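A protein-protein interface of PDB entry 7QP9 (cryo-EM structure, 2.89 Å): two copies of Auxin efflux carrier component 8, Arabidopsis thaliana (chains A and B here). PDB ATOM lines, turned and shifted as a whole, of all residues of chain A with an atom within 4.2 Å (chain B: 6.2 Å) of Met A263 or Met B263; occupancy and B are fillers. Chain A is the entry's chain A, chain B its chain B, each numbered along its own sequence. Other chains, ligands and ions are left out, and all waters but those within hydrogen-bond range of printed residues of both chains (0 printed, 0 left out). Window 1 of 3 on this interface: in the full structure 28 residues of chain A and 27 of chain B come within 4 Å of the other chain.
The backbone NH (N) of Ser B51 sits at hydrogen-bond distance from the backbone carbonyl oxygen (O) of Phe B46 (3.5 Å). O of Met A263 lies within hydrogen-bond range of OG of Ser A267 (2.8 Å). O of Met B263 lies within hydrogen-bond range of OG of Ser B267 (2.8 Å).
Of the 11 printed residues of chain A, 5 touch a printed residue of chain B. Hydrophobic or aromatic side chains of chain A within 4 Å of the printed part of chain B: Phe A46, Met A263 and Phe A266. Printed residues of chain B that touch a printed residue of chain A: Phe B46, Leu B255, Gly B259, Met B263 and Phe B266. Hydrophobic or aromatic side chains of chain B within 4 Å of the printed part of chain A: Phe B46, Leu B255, Met B263 and Phe B266. Among the printed residues, no Asp or Glu carboxylate lies within 4 Å of a Lys or Arg side-chain nitrogen of the other chain.
Phe A46 touches Phe B266, and with the chains exchanged Phe A266 touches Phe B46. Gly B259 touches its own counterpart, Gly A259. Met B263 touches its own counterpart, Met A263.
SD of Met A263 lies close to SD of Met B263.
Of the printed residues of chain B, Phe A46 touches Phe B266. Printed residues of chain B within 4 Å of Gly A259: Gly B259. Of the printed residues of chain B, Gly A262 touches Leu B255 (3.5 Å). Met A263 touches just one residue of chain B: Met B263. Printed residues of chain A within 4 Å of Phe B46: Phe A266. Printed residues of chain A within 4 Å of Leu B255: Gly A262. Met B263 touches one residue of chain A. The nearest residue of chain B that does not touch Met A263 is Phe B46 (4.3 Å).
CD1 of Phe A46 touches CE2 of Phe B266 (3.5 Å). Gly B259 touches Gly A259 (N to N, 3.8 Å). Gly A262 touches Leu B255 (CA to O, 3.5 Å). CD1 of Phe B46 touches CE2 of Phe A266 (3.5 Å).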
ATOM      1  N   PHE A  46       2.677 -21.538  -6.108  1.00  0.00           N
ATOM      2  CA  PHE A  46       2.996 -20.871  -4.852  1.00  0.00           C
ATOM      3  C   PHE A  46       1.745 -20.274  -4.225  1.00  0.00           C
ATOM      4  O   PHE A  46       1.544 -20.368  -3.010  1.00  0.00           O
ATOM      5  CB  PHE A  46       4.044 -19.782  -5.069  1.00  0.00           C
ATOM      6  CG  PHE A  46       4.310 -18.957  -3.843  1.00  0.00           C
ATOM      7  CD1 PHE A  46       5.230 -19.374  -2.899  1.00  0.00           C
ATOM      8  CD2 PHE A  46       3.627 -17.776  -3.623  1.00  0.00           C
ATOM      9  CE1 PHE A  46       5.469 -18.622  -1.769  1.00  0.00           C
ATOM     10  CE2 PHE A  46       3.864 -17.022  -2.494  1.00  0.00           C
ATOM     11  CZ  PHE A  46       4.785 -17.447  -1.566  1.00  0.00           C
ATOM     12  N   VAL A  47       0.893 -19.650  -5.038  1.00  0.00           N
ATOM     13  CA  VAL A  47      -0.344 -19.080  -4.508  1.00  0.00           C
ATOM     14  C   VAL A  47      -1.213 -20.173  -3.901  1.00  0.00           C
ATOM     15  O   VAL A  47      -1.809 -19.995  -2.833  1.00  0.00           O
ATOM     16  CB  VAL A  47      -1.096 -18.312  -5.610  1.00  0.00           C
ATOM     17  CG1 VAL A  47      -2.398 -17.749  -5.068  1.00  0.00           C
ATOM     18  CG2 VAL A  47      -0.229 -17.205  -6.168  1.00  0.00           C
ATOM     19  N   GLY A 259       0.530 -11.050   0.908  1.00  0.00           N
ATOM     20  CA  GLY A 259       0.325 -10.811  -0.507  1.00  0.00           C
ATOM     21  C   GLY A 259      -0.358 -11.964  -1.213  1.00  0.00           C
ATOM     22  O   GLY A 259       0.038 -12.340  -2.319  1.00  0.00           O
ATOM     23  N   GLY A 260      -1.385 -12.533  -0.590  1.00  0.00           N
ATOM     24  CA  GLY A 260      -2.058 -13.689  -1.150  1.00  0.00           C
ATOM     25  C   GLY A 260      -3.063 -13.347  -2.230  1.00  0.00           C
ATOM     26  O   GLY A 260      -3.002 -13.888  -3.338  1.00  0.00           O
ATOM     27  N   LEU A 261      -4.002 -12.454  -1.916  1.00  0.00           N
ATOM     28  CA  LEU A 261      -5.023 -12.083  -2.890  1.00  0.00           C
ATOM     29  C   LEU A 261      -4.407 -11.386  -4.096  1.00  0.00           C
ATOM     30  O   LEU A 261      -4.810 -11.633  -5.240  1.00  0.00           O
ATOM     31  CB  LEU A 261      -6.070 -11.186  -2.233  1.00  0.00           C
ATOM     32  CG  LEU A 261      -7.183 -10.684  -3.152  1.00  0.00           C
ATOM     33  CD1 LEU A 261      -8.038 -11.835  -3.657  1.00  0.00           C
ATOM     34  CD2 LEU A 261      -8.030  -9.667  -2.421  1.00  0.00           C
ATOM     35  N   GLY A 262      -3.445 -10.494  -3.860  1.00  0.00           N
ATOM     36  CA  GLY A 262      -2.791  -9.828  -4.971  1.00  0.00           C
ATOM     37  C   GLY A 262      -2.131 -10.810  -5.916  1.00  0.00           C
ATOM     38  O   GLY A 262      -2.242 -10.682  -7.137  1.00  0.00           O
ATOM     39  N   MET A 263      -1.452 -11.817  -5.365  1.00  0.00           N
ATOM     40  CA  MET A 263      -0.821 -12.825  -6.208  1.00  0.00           C
ATOM     41  C   MET A 263      -1.848 -13.711  -6.898  1.00  0.00           C
ATOM     42  O   MET A 263      -1.608 -14.167  -8.018  1.00  0.00           O
ATOM     43  CB  MET A 263       0.132 -13.681  -5.384  1.00  0.00           C
ATOM     44  CG  MET A 263       1.413 -12.984  -4.997  1.00  0.00           C
ATOM     45  SD  MET A 263       2.522 -14.118  -4.156  1.00  0.00           S
ATOM     46  CE  MET A 263       3.048 -15.127  -5.538  1.00  0.00           C
ATOM     47  N   ALA A 264      -2.982 -13.983  -6.252  1.00  0.00           N
ATOM     48  CA  ALA A 264      -4.029 -14.753  -6.913  1.00  0.00           C
ATOM     49  C   ALA A 264      -4.563 -14.011  -8.132  1.00  0.00           C
ATOM     50  O   ALA A 264      -4.742 -14.595  -9.208  1.00  0.00           O
ATOM     51  CB  ALA A 264      -5.156 -15.057  -5.927  1.00  0.00           C
ATOM     52  N   MET A 265      -4.810 -12.709  -7.984  1.00  0.00           N
ATOM     53  CA  MET A 265      -5.263 -11.915  -9.124  1.00  0.00           C
ATOM     54  C   MET A 265      -4.171 -11.811 -10.185  1.00  0.00           C
ATOM     55  O   MET A 265      -4.458 -11.827 -11.389  1.00  0.00           O
ATOM     56  CB  MET A 265      -5.698 -10.526  -8.660  1.00  0.00           C
ATOM     57  CG  MET A 265      -6.706 -10.520  -7.516  1.00  0.00           C
ATOM     58  SD  MET A 265      -8.191 -11.509  -7.778  1.00  0.00           S
ATOM     59  CE  MET A 265      -8.665 -11.020  -9.426  1.00  0.00           C
ATOM     60  N   PHE A 266      -2.912 -11.704  -9.756  1.00  0.00           N
ATOM     61  CA  PHE A 266      -1.799 -11.696 -10.699  1.00  0.00           C
ATOM     62  C   PHE A 266      -1.756 -12.985 -11.508  1.00  0.00           C
ATOM     63  O   PHE A 266      -1.531 -12.957 -12.721  1.00  0.00           O
ATOM     64  CB  PHE A 266      -0.490 -11.495  -9.936  1.00  0.00           C
ATOM     65  CG  PHE A 266       0.662 -11.082 -10.799  1.00  0.00           C
ATOM     66  CD1 PHE A 266       0.869  -9.752 -11.114  1.00  0.00           C
ATOM     67  CD2 PHE A 266       1.551 -12.026 -11.283  1.00  0.00           C
ATOM     68  CE1 PHE A 266       1.932  -9.375 -11.903  1.00  0.00           C
ATOM     69  CE2 PHE A 266       2.615 -11.653 -12.073  1.00  0.00           C
ATOM     70  CZ  PHE A 266       2.806 -10.327 -12.382  1.00  0.00           C
ATOM     71  N   SER A 267      -1.965 -14.125 -10.849  1.00  0.00           N
ATOM     72  CA  SER A 267      -1.979 -15.405 -11.548  1.00  0.00           C
ATOM     73  C   SER A 267      -3.164 -15.501 -12.496  1.00  0.00           C
ATOM     74  O   SER A 267      -3.055 -16.088 -13.579  1.00  0.00           O
ATOM     75  CB  SER A 267      -2.012 -16.547 -10.538  1.00  0.00           C
ATOM     76  OG  SER A 267      -1.001 -16.387  -9.561  1.00  0.00           O
ATOM     77  N   SER B  21      10.346 -18.085   6.457  1.00  0.00           N
ATOM     78  CA  SER B  21      10.083 -18.038   5.021  1.00  0.00           C
ATOM     79  C   SER B  21      11.226 -18.674   4.239  1.00  0.00           C
ATOM     80  O   SER B  21      10.999 -19.408   3.268  1.00  0.00           O
ATOM     81  CB  SER B  21       9.866 -16.596   4.571  1.00  0.00           C
ATOM     82  OG  SER B  21       8.655 -16.082   5.089  1.00  0.00           O
ATOM     83  N   ILE B  43       9.609 -16.956  -9.795  1.00  0.00           N
ATOM     84  CA  ILE B  43       9.257 -16.343  -8.516  1.00  0.00           C
ATOM     85  C   ILE B  43      10.232 -15.221  -8.182  1.00  0.00           C
ATOM     86  O   ILE B  43       9.829 -14.132  -7.746  1.00  0.00           O
ATOM     87  CB  ILE B  43       9.216 -17.411  -7.407  1.00  0.00           C
ATOM     88  CG1 ILE B  43       7.890 -18.170  -7.451  1.00  0.00           C
ATOM     89  CG2 ILE B  43       9.407 -16.778  -6.035  1.00  0.00           C
ATOM     90  CD1 ILE B  43       7.978 -19.576  -6.915  1.00  0.00           C
ATOM     91  N   PHE B  46       9.464 -12.226 -10.341  1.00  0.00           N
ATOM     92  CA  PHE B  46       8.310 -11.490  -9.835  1.00  0.00           C
ATOM     93  C   PHE B  46       8.695 -10.640  -8.634  1.00  0.00           C
ATOM     94  O   PHE B  46       8.266  -9.488  -8.516  1.00  0.00           O
ATOM     95  CB  PHE B  46       7.181 -12.448  -9.461  1.00  0.00           C
ATOM     96  CG  PHE B  46       6.013 -11.769  -8.809  1.00  0.00           C
ATOM     97  CD1 PHE B  46       5.015 -11.194  -9.573  1.00  0.00           C
ATOM     98  CD2 PHE B  46       5.918 -11.695  -7.432  1.00  0.00           C
ATOM     99  CE1 PHE B  46       3.945 -10.562  -8.975  1.00  0.00           C
ATOM    100  CE2 PHE B  46       4.850 -11.064  -6.832  1.00  0.00           C
ATOM    101  CZ  PHE B  46       3.863 -10.498  -7.605  1.00  0.00           C
ATOM    102  N   VAL B  47       9.504 -11.192  -7.729  1.00  0.00           N
ATOM    103  CA  VAL B  47       9.945 -10.415  -6.574  1.00  0.00           C
ATOM    104  C   VAL B  47      10.748  -9.201  -7.025  1.00  0.00           C
ATOM    105  O   VAL B  47      10.581  -8.095  -6.500  1.00  0.00           O
ATOM    106  CB  VAL B  47      10.754 -11.302  -5.608  1.00  0.00           C
ATOM    107  CG1 VAL B  47      11.201 -10.502  -4.397  1.00  0.00           C
ATOM    108  CG2 VAL B  47       9.934 -12.499  -5.175  1.00  0.00           C
ATOM    109  N   SER B  51       7.688  -6.761  -6.439  1.00  0.00           N
ATOM    110  CA  SER B  51       7.721  -6.625  -4.988  1.00  0.00           C
ATOM    111  C   SER B  51       8.702  -5.543  -4.558  1.00  0.00           C
ATOM    112  O   SER B  51       8.334  -4.604  -3.845  1.00  0.00           O
ATOM    113  CB  SER B  51       8.083  -7.965  -4.347  1.00  0.00           C
ATOM    114  OG  SER B  51       6.973  -8.845  -4.343  1.00  0.00           O
ATOM    115  N   LEU B 255      -1.683  -4.274  -2.420  1.00  0.00           N
ATOM    116  CA  LEU B 255      -2.138  -5.620  -2.746  1.00  0.00           C
ATOM    117  C   LEU B 255      -0.991  -6.476  -3.267  1.00  0.00           C
ATOM    118  O   LEU B 255      -0.878  -7.656  -2.918  1.00  0.00           O
ATOM    119  CB  LEU B 255      -3.268  -5.552  -3.773  1.00  0.00           C
ATOM    120  CG  LEU B 255      -4.257  -6.717  -3.782  1.00  0.00           C
ATOM    121  CD1 LEU B 255      -5.120  -6.696  -2.536  1.00  0.00           C
ATOM    122  CD2 LEU B 255      -5.122  -6.677  -5.026  1.00  0.00           C
ATOM    123  N   LEU B 256      -0.130  -5.899  -4.104  1.00  0.00           N
ATOM    124  CA  LEU B 256       0.977  -6.633  -4.699  1.00  0.00           C
ATOM    125  C   LEU B 256       2.286  -6.486  -3.935  1.00  0.00           C
ATOM    126  O   LEU B 256       3.155  -7.356  -4.061  1.00  0.00           O
ATOM    127  CB  LEU B 256       1.199  -6.174  -6.145  1.00  0.00           C
ATOM    128  CG  LEU B 256       0.472  -6.973  -7.226  1.00  0.00           C
ATOM    129  CD1 LEU B 256       0.544  -6.243  -8.553  1.00  0.00           C
ATOM    130  CD2 LEU B 256       1.050  -8.371  -7.355  1.00  0.00           C
ATOM    131  N   SER B 257       2.452  -5.420  -3.156  1.00  0.00           N
ATOM    132  CA  SER B 257       3.709  -5.174  -2.463  1.00  0.00           C
ATOM    133  C   SER B 257       3.729  -5.709  -1.039  1.00  0.00           C
ATOM    134  O   SER B 257       4.791  -5.705  -0.410  1.00  0.00           O
ATOM    135  CB  SER B 257       3.997  -3.672  -2.430  1.00  0.00           C
ATOM    136  OG  SER B 257       3.162  -3.017  -1.495  1.00  0.00           O
ATOM    137  N   ASP B 258       2.592  -6.169  -0.516  1.00  0.00           N
ATOM    138  CA  ASP B 258       2.526  -6.538   0.894  1.00  0.00           C
ATOM    139  C   ASP B 258       3.424  -7.729   1.206  1.00  0.00           C
ATOM    140  O   ASP B 258       4.061  -7.770   2.265  1.00  0.00           O
ATOM    141  CB  ASP B 258       1.081  -6.837   1.287  1.00  0.00           C
ATOM    142  CG  ASP B 258       0.381  -5.640   1.907  1.00  0.00           C
ATOM    143  OD1 ASP B 258       1.066  -4.781   2.500  1.00  0.00           O
ATOM    144  OD2 ASP B 258      -0.861  -5.563   1.804  1.00  0.00           O
ATOM    145  N   GLY B 259       3.486  -8.707   0.307  1.00  0.00           N
ATOM    146  CA  GLY B 259       4.252  -9.914   0.556  1.00  0.00           C
ATOM    147  C   GLY B 259       5.642  -9.893  -0.046  1.00  0.00           C
ATOM    148  O   GLY B 259       6.236 -10.950  -0.276  1.00  0.00           O
ATOM    149  N   GLY B 260       6.174  -8.699  -0.307  1.00  0.00           N
ATOM    150  CA  GLY B 260       7.453  -8.609  -0.995  1.00  0.00           C
ATOM    151  C   GLY B 260       8.592  -9.232  -0.211  1.00  0.00           C
ATOM    152  O   GLY B 260       9.396  -9.990  -0.757  1.00  0.00           O
ATOM    153  N   LEU B 261       8.681  -8.917   1.081  1.00  0.00           N
ATOM    154  CA  LEU B 261       9.791  -9.414   1.889  1.00  0.00           C
ATOM    155  C   LEU B 261       9.694 -10.921   2.104  1.00  0.00           C
ATOM    156  O   LEU B 261      10.703 -11.634   2.025  1.00  0.00           O
ATOM    157  CB  LEU B 261       9.822  -8.682   3.228  1.00  0.00           C
ATOM    158  CG  LEU B 261      10.853  -9.168   4.246  1.00  0.00           C
ATOM    159  CD1 LEU B 261      12.265  -9.018   3.705  1.00  0.00           C
ATOM    160  CD2 LEU B 261      10.687  -8.405   5.540  1.00  0.00           C
ATOM    161  N   GLY B 262       8.493 -11.418   2.398  1.00  0.00           N
ATOM    162  CA  GLY B 262       8.323 -12.850   2.557  1.00  0.00           C
ATOM    163  C   GLY B 262       8.697 -13.611   1.304  1.00  0.00           C
ATOM    164  O   GLY B 262       9.349 -14.654   1.370  1.00  0.00           O
ATOM    165  N   MET B 263       8.307 -13.089   0.139  1.00  0.00           N
ATOM    166  CA  MET B 263       8.670 -13.736  -1.116  1.00  0.00           C
ATOM    167  C   MET B 263      10.156 -13.604  -1.418  1.00  0.00           C
ATOM    168  O   MET B 263      10.732 -14.491  -2.048  1.00  0.00           O
ATOM    169  CB  MET B 263       7.843 -13.161  -2.260  1.00  0.00           C
ATOM    170  CG  MET B 263       6.366 -13.481  -2.164  1.00  0.00           C
ATOM    171  SD  MET B 263       5.438 -12.834  -3.561  1.00  0.00           S
ATOM    172  CE  MET B 263       5.411 -11.090  -3.163  1.00  0.00           C
ATOM    173  N   ALA B 264      10.795 -12.516  -0.984  1.00  0.00           N
ATOM    174  CA  ALA B 264      12.241 -12.411  -1.153  1.00  0.00           C
ATOM    175  C   ALA B 264      12.963 -13.482  -0.344  1.00  0.00           C
ATOM    176  O   ALA B 264      13.877 -14.148  -0.848  1.00  0.00           O
ATOM    177  CB  ALA B 264      12.714 -11.017  -0.745  1.00  0.00           C
ATOM    178  N   MET B 265      12.555 -13.671   0.912  1.00  0.00           N
ATOM    179  CA  MET B 265      13.145 -14.738   1.719  1.00  0.00           C
ATOM    180  C   MET B 265      12.820 -16.108   1.132  1.00  0.00           C
ATOM    181  O   MET B 265      13.656 -17.019   1.153  1.00  0.00           O
ATOM    182  CB  MET B 265      12.655 -14.641   3.163  1.00  0.00           C
ATOM    183  CG  MET B 265      12.858 -13.280   3.816  1.00  0.00           C
ATOM    184  SD  MET B 265      14.514 -12.598   3.617  1.00  0.00           S
ATOM    185  CE  MET B 265      15.518 -13.944   4.226  1.00  0.00           C
ATOM    186  N   PHE B 266      11.606 -16.271   0.604  1.00  0.00           N
ATOM    187  CA  PHE B 266      11.233 -17.523  -0.042  1.00  0.00           C
ATOM    188  C   PHE B 266      12.131 -17.813  -1.238  1.00  0.00           C
ATOM    189  O   PHE B 266      12.568 -18.950  -1.432  1.00  0.00           O
ATOM    190  CB  PHE B 266       9.769 -17.455  -0.473  1.00  0.00           C
ATOM    191  CG  PHE B 266       9.151 -18.792  -0.749  1.00  0.00           C
ATOM    192  CD1 PHE B 266       8.621 -19.550   0.278  1.00  0.00           C
ATOM    193  CD2 PHE B 266       9.090 -19.286  -2.040  1.00  0.00           C
ATOM    194  CE1 PHE B 266       8.050 -20.774   0.025  1.00  0.00           C
ATOM    195  CE2 PHE B 266       8.519 -20.513  -2.298  1.00  0.00           C
ATOM    196  CZ  PHE B 266       7.999 -21.257  -1.265  1.00  0.00           C
ATOM    197  N   SER B 267      12.411 -16.795  -2.053  1.00  0.00           N
ATOM    198  CA  SER B 267      13.293 -16.970  -3.200  1.00  0.00           C
ATOM    199  C   SER B 267      14.712 -17.294  -2.757  1.00  0.00           C
ATOM    200  O   SER B 267      15.406 -18.086  -3.404  1.00  0.00           O
ATOM    201  CB  SER B 267      13.281 -15.709  -4.061  1.00  0.00           C
ATOM    202  OG  SER B 267      11.956 -15.329  -4.378  1.00  0.00           O
ATOM    203  N   LEU B 268      15.168 -16.677  -1.667  1.00  0.00           N
ATOM    204  CA  LEU B 268      16.485 -17.010  -1.133  1.00  0.00           C
ATOM    205  C   LEU B 268      16.548 -18.475  -0.718  1.00  0.00           C
ATOM    206  O   LEU B 268      17.525 -19.175  -1.004  1.00  0.00           O
ATOM    207  CB  LEU B 268      16.812 -16.087   0.040  1.00  0.00           C
ATOM    208  CG  LEU B 268      18.093 -16.348   0.830  1.00  0.00           C
ATOM    209  CD1 LEU B 268      19.252 -16.675  -0.081  1.00  0.00           C
ATOM    210  CD2 LEU B 268      18.425 -15.133   1.669  1.00  0.00           C
